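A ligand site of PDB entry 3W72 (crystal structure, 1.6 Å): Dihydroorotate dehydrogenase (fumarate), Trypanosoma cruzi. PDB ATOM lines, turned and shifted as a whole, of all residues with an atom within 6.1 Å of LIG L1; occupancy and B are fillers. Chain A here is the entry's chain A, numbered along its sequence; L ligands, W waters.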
ATOM      1  N   ALA A  20     -18.189   3.082  12.922  1.00  0.00           N
ATOM      2  CA  ALA A  20     -18.491   2.163  13.955  1.00  0.00           C
ATOM      3  C   ALA A  20     -19.225   2.798  15.110  1.00  0.00           C
ATOM      4  O   ALA A  20     -18.919   3.942  15.509  1.00  0.00           O
ATOM      5  CB  ALA A  20     -17.225   1.445  14.431  1.00  0.00           C
ATOM      6  N   LYS A  44     -20.861  -2.540  15.404  1.00  0.00           N
ATOM      7  CA  LYS A  44     -20.472  -1.866  16.638  1.00  0.00           C
ATOM      8  C   LYS A  44     -19.248  -2.584  17.243  1.00  0.00           C
ATOM      9  O   LYS A  44     -19.231  -3.834  17.345  1.00  0.00           O
ATOM     10  CB  LYS A  44     -21.659  -2.029  17.618  1.00  0.00           C
ATOM     11  CG  LYS A  44     -21.424  -1.612  19.035  1.00  0.00           C
ATOM     12  CD  LYS A  44     -21.132  -0.102  19.258  1.00  0.00           C
ATOM     13  CE  LYS A  44     -20.653   0.354  20.639  1.00  0.00           C
ATOM     14  NZ  LYS A  44     -20.255   1.838  20.703  1.00  0.00           N
ATOM     15  N   SER A  45     -18.337  -1.788  17.772  1.00  0.00           N
ATOM     16  CA  SER A  45     -17.123  -2.376  18.440  1.00  0.00           C
ATOM     17  C   SER A  45     -17.663  -3.256  19.572  1.00  0.00           C
ATOM     18  O   SER A  45     -18.461  -2.846  20.384  1.00  0.00           O
ATOM     19  CB  SER A  45     -16.225  -1.339  19.057  1.00  0.00           C
ATOM     20  OG  SER A  45     -15.633  -0.587  17.987  1.00  0.00           O
ATOM     21  N   THR A  47     -17.116  -6.451  22.677  1.00  0.00           N
ATOM     22  CA  THR A  47     -16.408  -7.172  23.703  1.00  0.00           C
ATOM     23  C   THR A  47     -16.821  -8.614  23.671  1.00  0.00           C
ATOM     24  O   THR A  47     -17.849  -8.979  23.094  1.00  0.00           O
ATOM     25  CB  THR A  47     -16.676  -6.523  25.095  1.00  0.00           C
ATOM     26  OG1 THR A  47     -18.063  -6.245  25.253  1.00  0.00           O
ATOM     27  CG2 THR A  47     -15.891  -5.261  25.291  1.00  0.00           C
ATOM     28  N   ARG A  51     -22.555  -5.888  26.803  1.00  0.00           N
ATOM     29  CA  ARG A  51     -22.533  -4.771  27.703  1.00  0.00           C
ATOM     30  C   ARG A  51     -23.767  -3.935  27.541  1.00  0.00           C
ATOM     31  O   ARG A  51     -24.204  -3.596  26.458  1.00  0.00           O
ATOM     32  CB  ARG A  51     -21.316  -3.860  27.430  1.00  0.00           C
ATOM     33  CG  ARG A  51     -20.018  -4.491  27.658  1.00  0.00           C
ATOM     34  CD  ARG A  51     -18.832  -3.652  27.277  1.00  0.00           C
ATOM     35  NE  ARG A  51     -18.814  -2.325  27.882  1.00  0.00           N
ATOM     36  CZ  ARG A  51     -18.228  -2.046  29.006  1.00  0.00           C
ATOM     37  NH1 ARG A  51     -17.550  -2.987  29.657  1.00  0.00           N
ATOM     38  NH2 ARG A  51     -18.192  -0.813  29.480  1.00  0.00           N
ATOM     39  N   ASN A  54     -23.293   2.707  29.474  1.00  0.00           N
ATOM     40  CA  ASN A  54     -23.505   3.705  30.511  1.00  0.00           C
ATOM     41  C   ASN A  54     -24.910   4.123  30.608  1.00  0.00           C
ATOM     42  O   ASN A  54     -25.738   3.990  29.729  1.00  0.00           O
ATOM     43  CB  ASN A  54     -22.626   4.906  30.153  1.00  0.00           C
ATOM     44  CG  ASN A  54     -21.190   4.677  30.416  1.00  0.00           C
ATOM     45  OD1 ASN A  54     -20.797   3.781  31.214  1.00  0.00           O
ATOM     46  ND2 ASN A  54     -20.353   5.451  29.811  1.00  0.00           N
ATOM     47  N   ASN A  68     -20.554  11.972  23.035  1.00  0.00           N
ATOM     48  CA  ASN A  68     -21.022  10.662  23.550  1.00  0.00           C
ATOM     49  C   ASN A  68     -20.041  10.090  24.504  1.00  0.00           C
ATOM     50  O   ASN A  68     -18.816  10.155  24.420  1.00  0.00           O
ATOM     51  CB  ASN A  68     -21.277   9.681  22.417  1.00  0.00           C
ATOM     52  CG  ASN A  68     -20.081   8.877  22.043  1.00  0.00           C
ATOM     53  OD1 ASN A  68     -19.644   7.874  22.644  1.00  0.00           O
ATOM     54  ND2 ASN A  68     -19.410   9.363  21.004  1.00  0.00           N
ATOM     55  N   SER A  69     -20.676   9.407  25.519  1.00  0.00           N
ATOM     56  CA  SER A  69     -19.936   8.477  26.416  1.00  0.00           C
ATOM     57  C   SER A  69     -20.774   7.219  26.550  1.00  0.00           C
ATOM     58  O   SER A  69     -21.420   7.051  27.552  1.00  0.00           O
ATOM     59  CB  SER A  69     -19.575   9.104  27.740  1.00  0.00           C
ATOM     60  OG  SER A  69     -18.535  10.098  27.558  1.00  0.00           O
ATOM     61  N   MET A  70     -20.886   6.447  25.492  1.00  0.00           N
ATOM     62  CA  MET A  70     -21.796   5.310  25.467  1.00  0.00           C
ATOM     63  C   MET A  70     -21.444   4.252  26.408  1.00  0.00           C
ATOM     64  O   MET A  70     -22.373   3.605  26.875  1.00  0.00           O
ATOM     65  CB  MET A  70     -21.875   4.780  24.061  1.00  0.00           C
ATOM     66  CG  MET A  70     -22.223   5.713  22.951  1.00  0.00           C
ATOM     67  SD  MET A  70     -23.820   6.513  23.105  1.00  0.00           S
ATOM     68  CE  MET A  70     -24.907   5.271  22.731  1.00  0.00           C
ATOM     69  N   GLY A  71     -20.180   4.055  26.662  1.00  0.00           N
ATOM     70  CA  GLY A  71     -19.704   2.933  27.485  1.00  0.00           C
ATOM     71  C   GLY A  71     -19.740   1.602  26.808  1.00  0.00           C
ATOM     72  O   GLY A  71     -19.817   0.574  27.451  1.00  0.00           O
ATOM     73  N   LEU A  72     -19.565   1.653  25.498  1.00  0.00           N
ATOM     74  CA  LEU A  72     -19.504   0.474  24.660  1.00  0.00           C
ATOM     75  C   LEU A  72     -20.684  -0.496  24.889  1.00  0.00           C
ATOM     76  O   LEU A  72     -20.459  -1.707  25.072  1.00  0.00           O
ATOM     77  CB  LEU A  72     -18.139  -0.245  24.726  1.00  0.00           C
ATOM     78  CG  LEU A  72     -17.966  -1.098  23.498  1.00  0.00           C
ATOM     79  CD1 LEU A  72     -17.314  -0.342  22.347  1.00  0.00           C
ATOM     80  CD2 LEU A  72     -17.067  -2.308  23.810  1.00  0.00           C
ATOM     81  N   PRO A  73     -21.891  -0.033  24.768  1.00  0.00           N
ATOM     82  CA  PRO A  73     -23.043  -0.955  24.780  1.00  0.00           C
ATOM     83  C   PRO A  73     -22.920  -1.795  23.542  1.00  0.00           C
ATOM     84  O   PRO A  73     -22.744  -1.281  22.425  1.00  0.00           O
ATOM     85  CB  PRO A  73     -24.268  -0.081  24.677  1.00  0.00           C
ATOM     86  CG  PRO A  73     -23.751   1.232  24.171  1.00  0.00           C
ATOM     87  CD  PRO A  73     -22.290   1.332  24.389  1.00  0.00           C
ATOM     88  N   SER A 100     -13.223  -4.320  20.200  1.00  0.00           N
ATOM     89  CA  SER A 100     -12.538  -3.483  21.159  1.00  0.00           C
ATOM     90  C   SER A 100     -12.664  -4.160  22.520  1.00  0.00           C
ATOM     91  O   SER A 100     -13.369  -3.738  23.371  1.00  0.00           O
ATOM     92  CB  SER A 100     -13.085  -2.036  21.139  1.00  0.00           C
ATOM     93  OG  SER A 100     -12.010  -1.149  21.502  1.00  0.00           O
ATOM     94  N   GLY A 101     -11.825  -5.171  22.701  1.00  0.00           N
ATOM     95  CA  GLY A 101     -11.650  -5.823  24.024  1.00  0.00           C
ATOM     96  C   GLY A 101     -11.041  -4.945  25.055  1.00  0.00           C
ATOM     97  O   GLY A 101     -10.360  -3.989  24.754  1.00  0.00           O
ATOM     98  N   LEU A 102     -11.257  -5.336  26.330  1.00  0.00           N
ATOM     99  CA  LEU A 102     -10.758  -4.545  27.481  1.00  0.00           C
ATOM    100  C   LEU A 102      -9.315  -4.947  27.832  1.00  0.00           C
ATOM    101  O   LEU A 102      -8.705  -4.306  28.680  1.00  0.00           O
ATOM    102  CB  LEU A 102     -11.647  -4.737  28.685  1.00  0.00           C
ATOM    103  CG  LEU A 102     -12.848  -3.812  28.951  1.00  0.00           C
ATOM    104  CD1 LEU A 102     -13.608  -3.381  27.748  1.00  0.00           C
ATOM    105  CD2 LEU A 102     -13.787  -4.530  29.922  1.00  0.00           C
ATOM    106  N   ASN A 128     -10.409  -1.539  17.105  1.00  0.00           N
ATOM    107  CA  ASN A 128     -10.553  -0.227  17.723  1.00  0.00           C
ATOM    108  C   ASN A 128      -9.531  -0.060  18.803  1.00  0.00           C
ATOM    109  O   ASN A 128      -9.700  -0.629  19.861  1.00  0.00           O
ATOM    110  CB  ASN A 128     -11.980  -0.064  18.229  1.00  0.00           C
ATOM    111  CG  ASN A 128     -12.257   1.215  18.979  1.00  0.00           C
ATOM    112  OD1 ASN A 128     -11.399   2.059  19.098  1.00  0.00           O
ATOM    113  ND2 ASN A 128     -13.489   1.390  19.434  1.00  0.00           N
ATOM    114  N   SER A 130      -8.857   2.629  20.575  1.00  0.00           N
ATOM    115  CA  SER A 130      -9.297   3.565  21.664  1.00  0.00           C
ATOM    116  C   SER A 130      -9.870   2.802  22.832  1.00  0.00           C
ATOM    117  O   SER A 130     -10.815   3.202  23.410  1.00  0.00           O
ATOM    118  CB  SER A 130     -10.226   4.648  21.095  1.00  0.00           C
ATOM    119  OG  SER A 130      -9.468   5.535  20.311  1.00  0.00           O
ATOM    120  N   CYS A 131      -9.344   1.641  23.111  1.00  0.00           N
ATOM    121  CA  CYS A 131      -9.789   0.774  24.180  1.00  0.00           C
ATOM    122  C   CYS A 131      -8.951   1.011  25.450  1.00  0.00           C
ATOM    123  O   CYS A 131      -7.855   1.660  25.465  1.00  0.00           O
ATOM    124  CB  CYS A 131      -9.663  -0.668  23.756  1.00  0.00           C
ATOM    125  SG  CYS A 131      -8.059  -0.999  22.971  1.00  0.00           S
ATOM    126  N   PRO A 132      -9.482   0.484  26.545  1.00  0.00           N
ATOM    127  CA  PRO A 132      -8.856   0.926  27.756  1.00  0.00           C
ATOM    128  C   PRO A 132      -7.592   0.162  28.026  1.00  0.00           C
ATOM    129  O   PRO A 132      -7.290  -0.935  27.490  1.00  0.00           O
ATOM    130  CB  PRO A 132      -9.887   0.616  28.851  1.00  0.00           C
ATOM    131  CG  PRO A 132     -10.888  -0.321  28.258  1.00  0.00           C
ATOM    132  CD  PRO A 132     -10.864  -0.010  26.768  1.00  0.00           C
ATOM    133  N   LYS A 165      -8.688   1.306  13.912  1.00  0.00           N
ATOM    134  CA  LYS A 165      -9.343   2.556  14.089  1.00  0.00           C
ATOM    135  C   LYS A 165      -8.558   3.333  15.132  1.00  0.00           C
ATOM    136  O   LYS A 165      -8.345   2.864  16.271  1.00  0.00           O
ATOM    137  CB  LYS A 165     -10.706   2.287  14.593  1.00  0.00           C
ATOM    138  CG  LYS A 165     -11.573   3.510  15.012  1.00  0.00           C
ATOM    139  CD  LYS A 165     -12.099   4.226  13.809  1.00  0.00           C
ATOM    140  CE  LYS A 165     -13.134   5.283  14.107  1.00  0.00           C
ATOM    141  NZ  LYS A 165     -14.444   4.728  14.417  1.00  0.00           N
ATOM    142  N   ASN A 195     -11.390   8.306  15.263  1.00  0.00           N
ATOM    143  CA  ASN A 195     -12.390   8.234  16.359  1.00  0.00           C
ATOM    144  C   ASN A 195     -12.714   9.637  16.883  1.00  0.00           C
ATOM    145  O   ASN A 195     -12.150  10.618  16.410  1.00  0.00           O
ATOM    146  CB  ASN A 195     -11.810   7.270  17.414  1.00  0.00           C
ATOM    147  CG  ASN A 195     -12.896   6.471  18.107  1.00  0.00           C
ATOM    148  OD1 ASN A 195     -13.959   6.998  18.471  1.00  0.00           O
ATOM    149  ND2 ASN A 195     -12.626   5.227  18.290  1.00  0.00           N
ATOM    150  N   SER A 196     -13.654   9.696  17.784  1.00  0.00           N
ATOM    151  CA  SER A 196     -14.027  10.951  18.310  1.00  0.00           C
ATOM    152  C   SER A 196     -12.886  11.697  18.965  1.00  0.00           C
ATOM    153  O   SER A 196     -11.941  11.146  19.415  1.00  0.00           O
ATOM    154  CB  SER A 196     -15.268  10.805  19.214  1.00  0.00           C
ATOM    155  OG  SER A 196     -15.113   9.834  20.140  1.00  0.00           O
ATOM    156  N   GLY A 220     -16.753  11.998  23.979  1.00  0.00           N
ATOM    157  CA  GLY A 220     -16.076  12.185  22.668  1.00  0.00           C
ATOM    158  C   GLY A 220     -16.882  13.012  21.763  1.00  0.00           C
ATOM    159  O   GLY A 220     -18.108  12.854  21.627  1.00  0.00           O
HETATM  160  O1  LIG L   1     -18.383   5.199  24.249  1.00  0.00           O
HETATM  161  C1  LIG L   1     -18.263   4.367  23.350  1.00  0.00           C
HETATM  162  O2  LIG L   1     -18.980   3.353  23.070  1.00  0.00           O
HETATM  163  C2  LIG L   1     -17.347   4.827  22.239  1.00  0.00           C
HETATM  164  N1  LIG L   1     -17.589   6.128  21.704  1.00  0.00           N
HETATM  165  C3  LIG L   1     -16.718   6.675  20.742  1.00  0.00           C
HETATM  166  O3  LIG L   1     -16.970   7.835  20.293  1.00  0.00           O
HETATM  167  N2  LIG L   1     -15.723   5.947  20.271  1.00  0.00           N
HETATM  168  C4  LIG L   1     -15.441   4.634  20.739  1.00  0.00           C
HETATM  169  O4  LIG L   1     -14.449   4.066  20.230  1.00  0.00           O
HETATM  170  C5  LIG L   1     -16.257   4.108  21.824  1.00  0.00           C
HETATM  171  C6  LIG L   1     -15.897   2.812  22.443  1.00  0.00           C
HETATM  172  C7  LIG L   1     -14.516   2.914  23.160  1.00  0.00           C
HETATM  173  C8  LIG L   1     -14.366   1.770  24.096  1.00  0.00           C
HETATM  174  C9  LIG L   1     -14.924   1.763  25.415  1.00  0.00           C
HETATM  175  C10 LIG L   1     -15.589   2.856  25.909  1.00  0.00           C
HETATM  176  C11 LIG L   1     -16.169   2.812  27.195  1.00  0.00           C
HETATM  177  C12 LIG L   1     -16.012   1.624  27.962  1.00  0.00           C
HETATM  178  C13 LIG L   1     -15.375   0.529  27.469  1.00  0.00           C
HETATM  179  C14 LIG L   1     -14.747   0.612  26.191  1.00  0.00           C
HETATM  180  C15 LIG L   1     -14.085  -0.472  25.664  1.00  0.00           C
HETATM  181  C16 LIG L   1     -13.420  -0.477  24.455  1.00  0.00           C
HETATM  182  C17 LIG L   1     -13.610   0.657  23.681  1.00  0.00           C
HETATM  183  N1  LG2 L   2     -16.063   4.346  17.152  1.00  0.00           N
HETATM  184  C1  LG2 L   2     -15.621   3.077  17.225  1.00  0.00           C
HETATM  185  O1  LG2 L   2     -14.632   2.721  16.572  1.00  0.00           O
HETATM  186  N2  LG2 L   2     -16.348   2.136  17.858  1.00  0.00           N
HETATM  187  C2  LG2 L   2     -17.478   2.387  18.418  1.00  0.00           C
HETATM  188  O2  LG2 L   2     -18.153   1.476  19.015  1.00  0.00           O
HETATM  189  C3  LG2 L   2     -18.004   3.734  18.452  1.00  0.00           C
HETATM  190  N3  LG2 L   2     -19.149   4.062  19.065  1.00  0.00           N
HETATM  191  C4  LG2 L   2     -19.697   5.227  18.782  1.00  0.00           C
HETATM  192  C5  LG2 L   2     -20.936   5.571  19.244  1.00  0.00           C
HETATM  193  C6  LG2 L   2     -21.546   6.759  19.009  1.00  0.00           C
HETATM  194  C7  LG2 L   2     -22.916   7.082  19.539  1.00  0.00           C
HETATM  195  C8  LG2 L   2     -20.825   7.730  18.300  1.00  0.00           C
HETATM  196  C9  LG2 L   2     -21.347   9.056  17.978  1.00  0.00           C
HETATM  197  C10 LG2 L   2     -19.544   7.435  17.849  1.00  0.00           C
HETATM  198  C11 LG2 L   2     -18.941   6.229  18.074  1.00  0.00           C
HETATM  199  N4  LG2 L   2     -17.684   5.937  17.596  1.00  0.00           N
HETATM  200  C12 LG2 L   2     -17.176   4.691  17.725  1.00  0.00           C
HETATM  201  C13 LG2 L   2     -16.864   6.924  16.873  1.00  0.00           C
HETATM  202  C14 LG2 L   2     -17.344   7.051  15.473  1.00  0.00           C
HETATM  203  O3  LG2 L   2     -17.096   5.831  14.755  1.00  0.00           O
HETATM  204  C15 LG2 L   2     -16.595   8.148  14.727  1.00  0.00           C
HETATM  205  O4  LG2 L   2     -15.176   7.846  14.729  1.00  0.00           O
HETATM  206  C16 LG2 L   2     -16.756   9.525  15.358  1.00  0.00           C
HETATM  207  O5  LG2 L   2     -18.107   9.742  15.743  1.00  0.00           O
HETATM  208  C17 LG2 L   2     -16.276  10.622  14.347  1.00  0.00           C
HETATM  209  O6  LG2 L   2     -17.100  10.670  13.195  1.00  0.00           O
HETATM  210  P1  LG2 L   2     -18.265  11.736  12.950  1.00  0.00           P
HETATM  211  O7  LG2 L   2     -18.814  11.386  11.665  1.00  0.00           O
HETATM  212  O8  LG2 L   2     -17.668  13.098  13.032  1.00  0.00           O
HETATM  213  O9  LG2 L   2     -19.212  11.521  14.110  1.00  0.00           O
HETATM  214  O   HOH W   1     -18.029   6.108  27.395  1.00  0.00           O
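A nitrogen (N2) of LIG L1 is in hydrogen-bond range of the side-chain amide oxygen of Asn 195 (2.7 Å).
The side-chain hydroxyl (OG) of Ser 45 sits at hydrogen-bond distance from a nitrogen (N2) of LG2 L2 (2.8 Å).
The backbone NH (N) of Gly 71 is in hydrogen-bond range of an oxygen (O1) of LIG L1 (3.2 Å).
The side-chain amino group (NZ) of Lys 165 sits at hydrogen-bond distance from an oxygen (O3) of LG2 L2 (2.9 Å).
NZ of Lys 44 sits at hydrogen-bond distance from O2 of LG2 L2 (2.7 Å).
N of Leu 72 is in hydrogen-bond range of O2 of LIG L1.
OG of Ser 196 sits at hydrogen-bond distance from O3 of LIG L1 (2.7 Å).
N2 of LG2 L2 sits close to ND2 of Asn 128, at 3.3 Å.
The side-chain amide nitrogen of Asn 128 is in hydrogen-bond range of an oxygen (O4) of LIG L1 (3.0 Å).
The backbone NH (N) of Ser 45 lies close to an oxygen (O2) of LG2 L2 (3.5 Å).
N of Met 70 sits at hydrogen-bond distance from O1 of LIG L1 (3.1 Å).
O2 of LIG L1 is in salt-bridge range of NZ of Lys 44.
N1 of LIG L1 sits at hydrogen-bond distance from OD1 of Asn 68 (2.9 Å).
O3 of LG2 L2 is in hydrogen-bond range of N of Ala 20 (3.5 Å).
O of Ala 20 lies within hydrogen-bond range of O3 of LG2 L2 (2.7 Å).
Residues that only touch LIG L1: Arg 51 (3.6 Å), Ser 69 (3.9 Å), Ser 100 (3.3 Å), Leu 102 (3.6 Å), Ser 130 (3.7 Å), Cys 131 (3.8 Å) and Pro 132 (3.4 Å).
Of the 23 residues printed, 15 come within 4 Å of LIG L1.
N of Gly 71 lies close to ND2 of Asn 54 (3.4 Å).
N of Gly 220 is in hydrogen-bond range of O of Asn 68.
OD1 of Asn 195 lies within hydrogen-bond range of OG of Ser 196 (3.5 Å).
The side-chain sulfur (SG) of Cys 131 is in hydrogen-bond range of the backbone carbonyl oxygen (O) of Asn 128 (3.5 Å).
The side-chain amide oxygen (OD1) of Asn 68 sits close to the backbone NH (N) of Met 70 (3.4 Å).
O of Leu 72 sits close to NE of Arg 51, 3.3 Å away.
OD1 of Asn 128 lies within hydrogen-bond range of N of Ser 130, at 3.0 Å.
O of Ser 69 is in hydrogen-bond range of ND2 of Asn 54 (3.0 Å).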
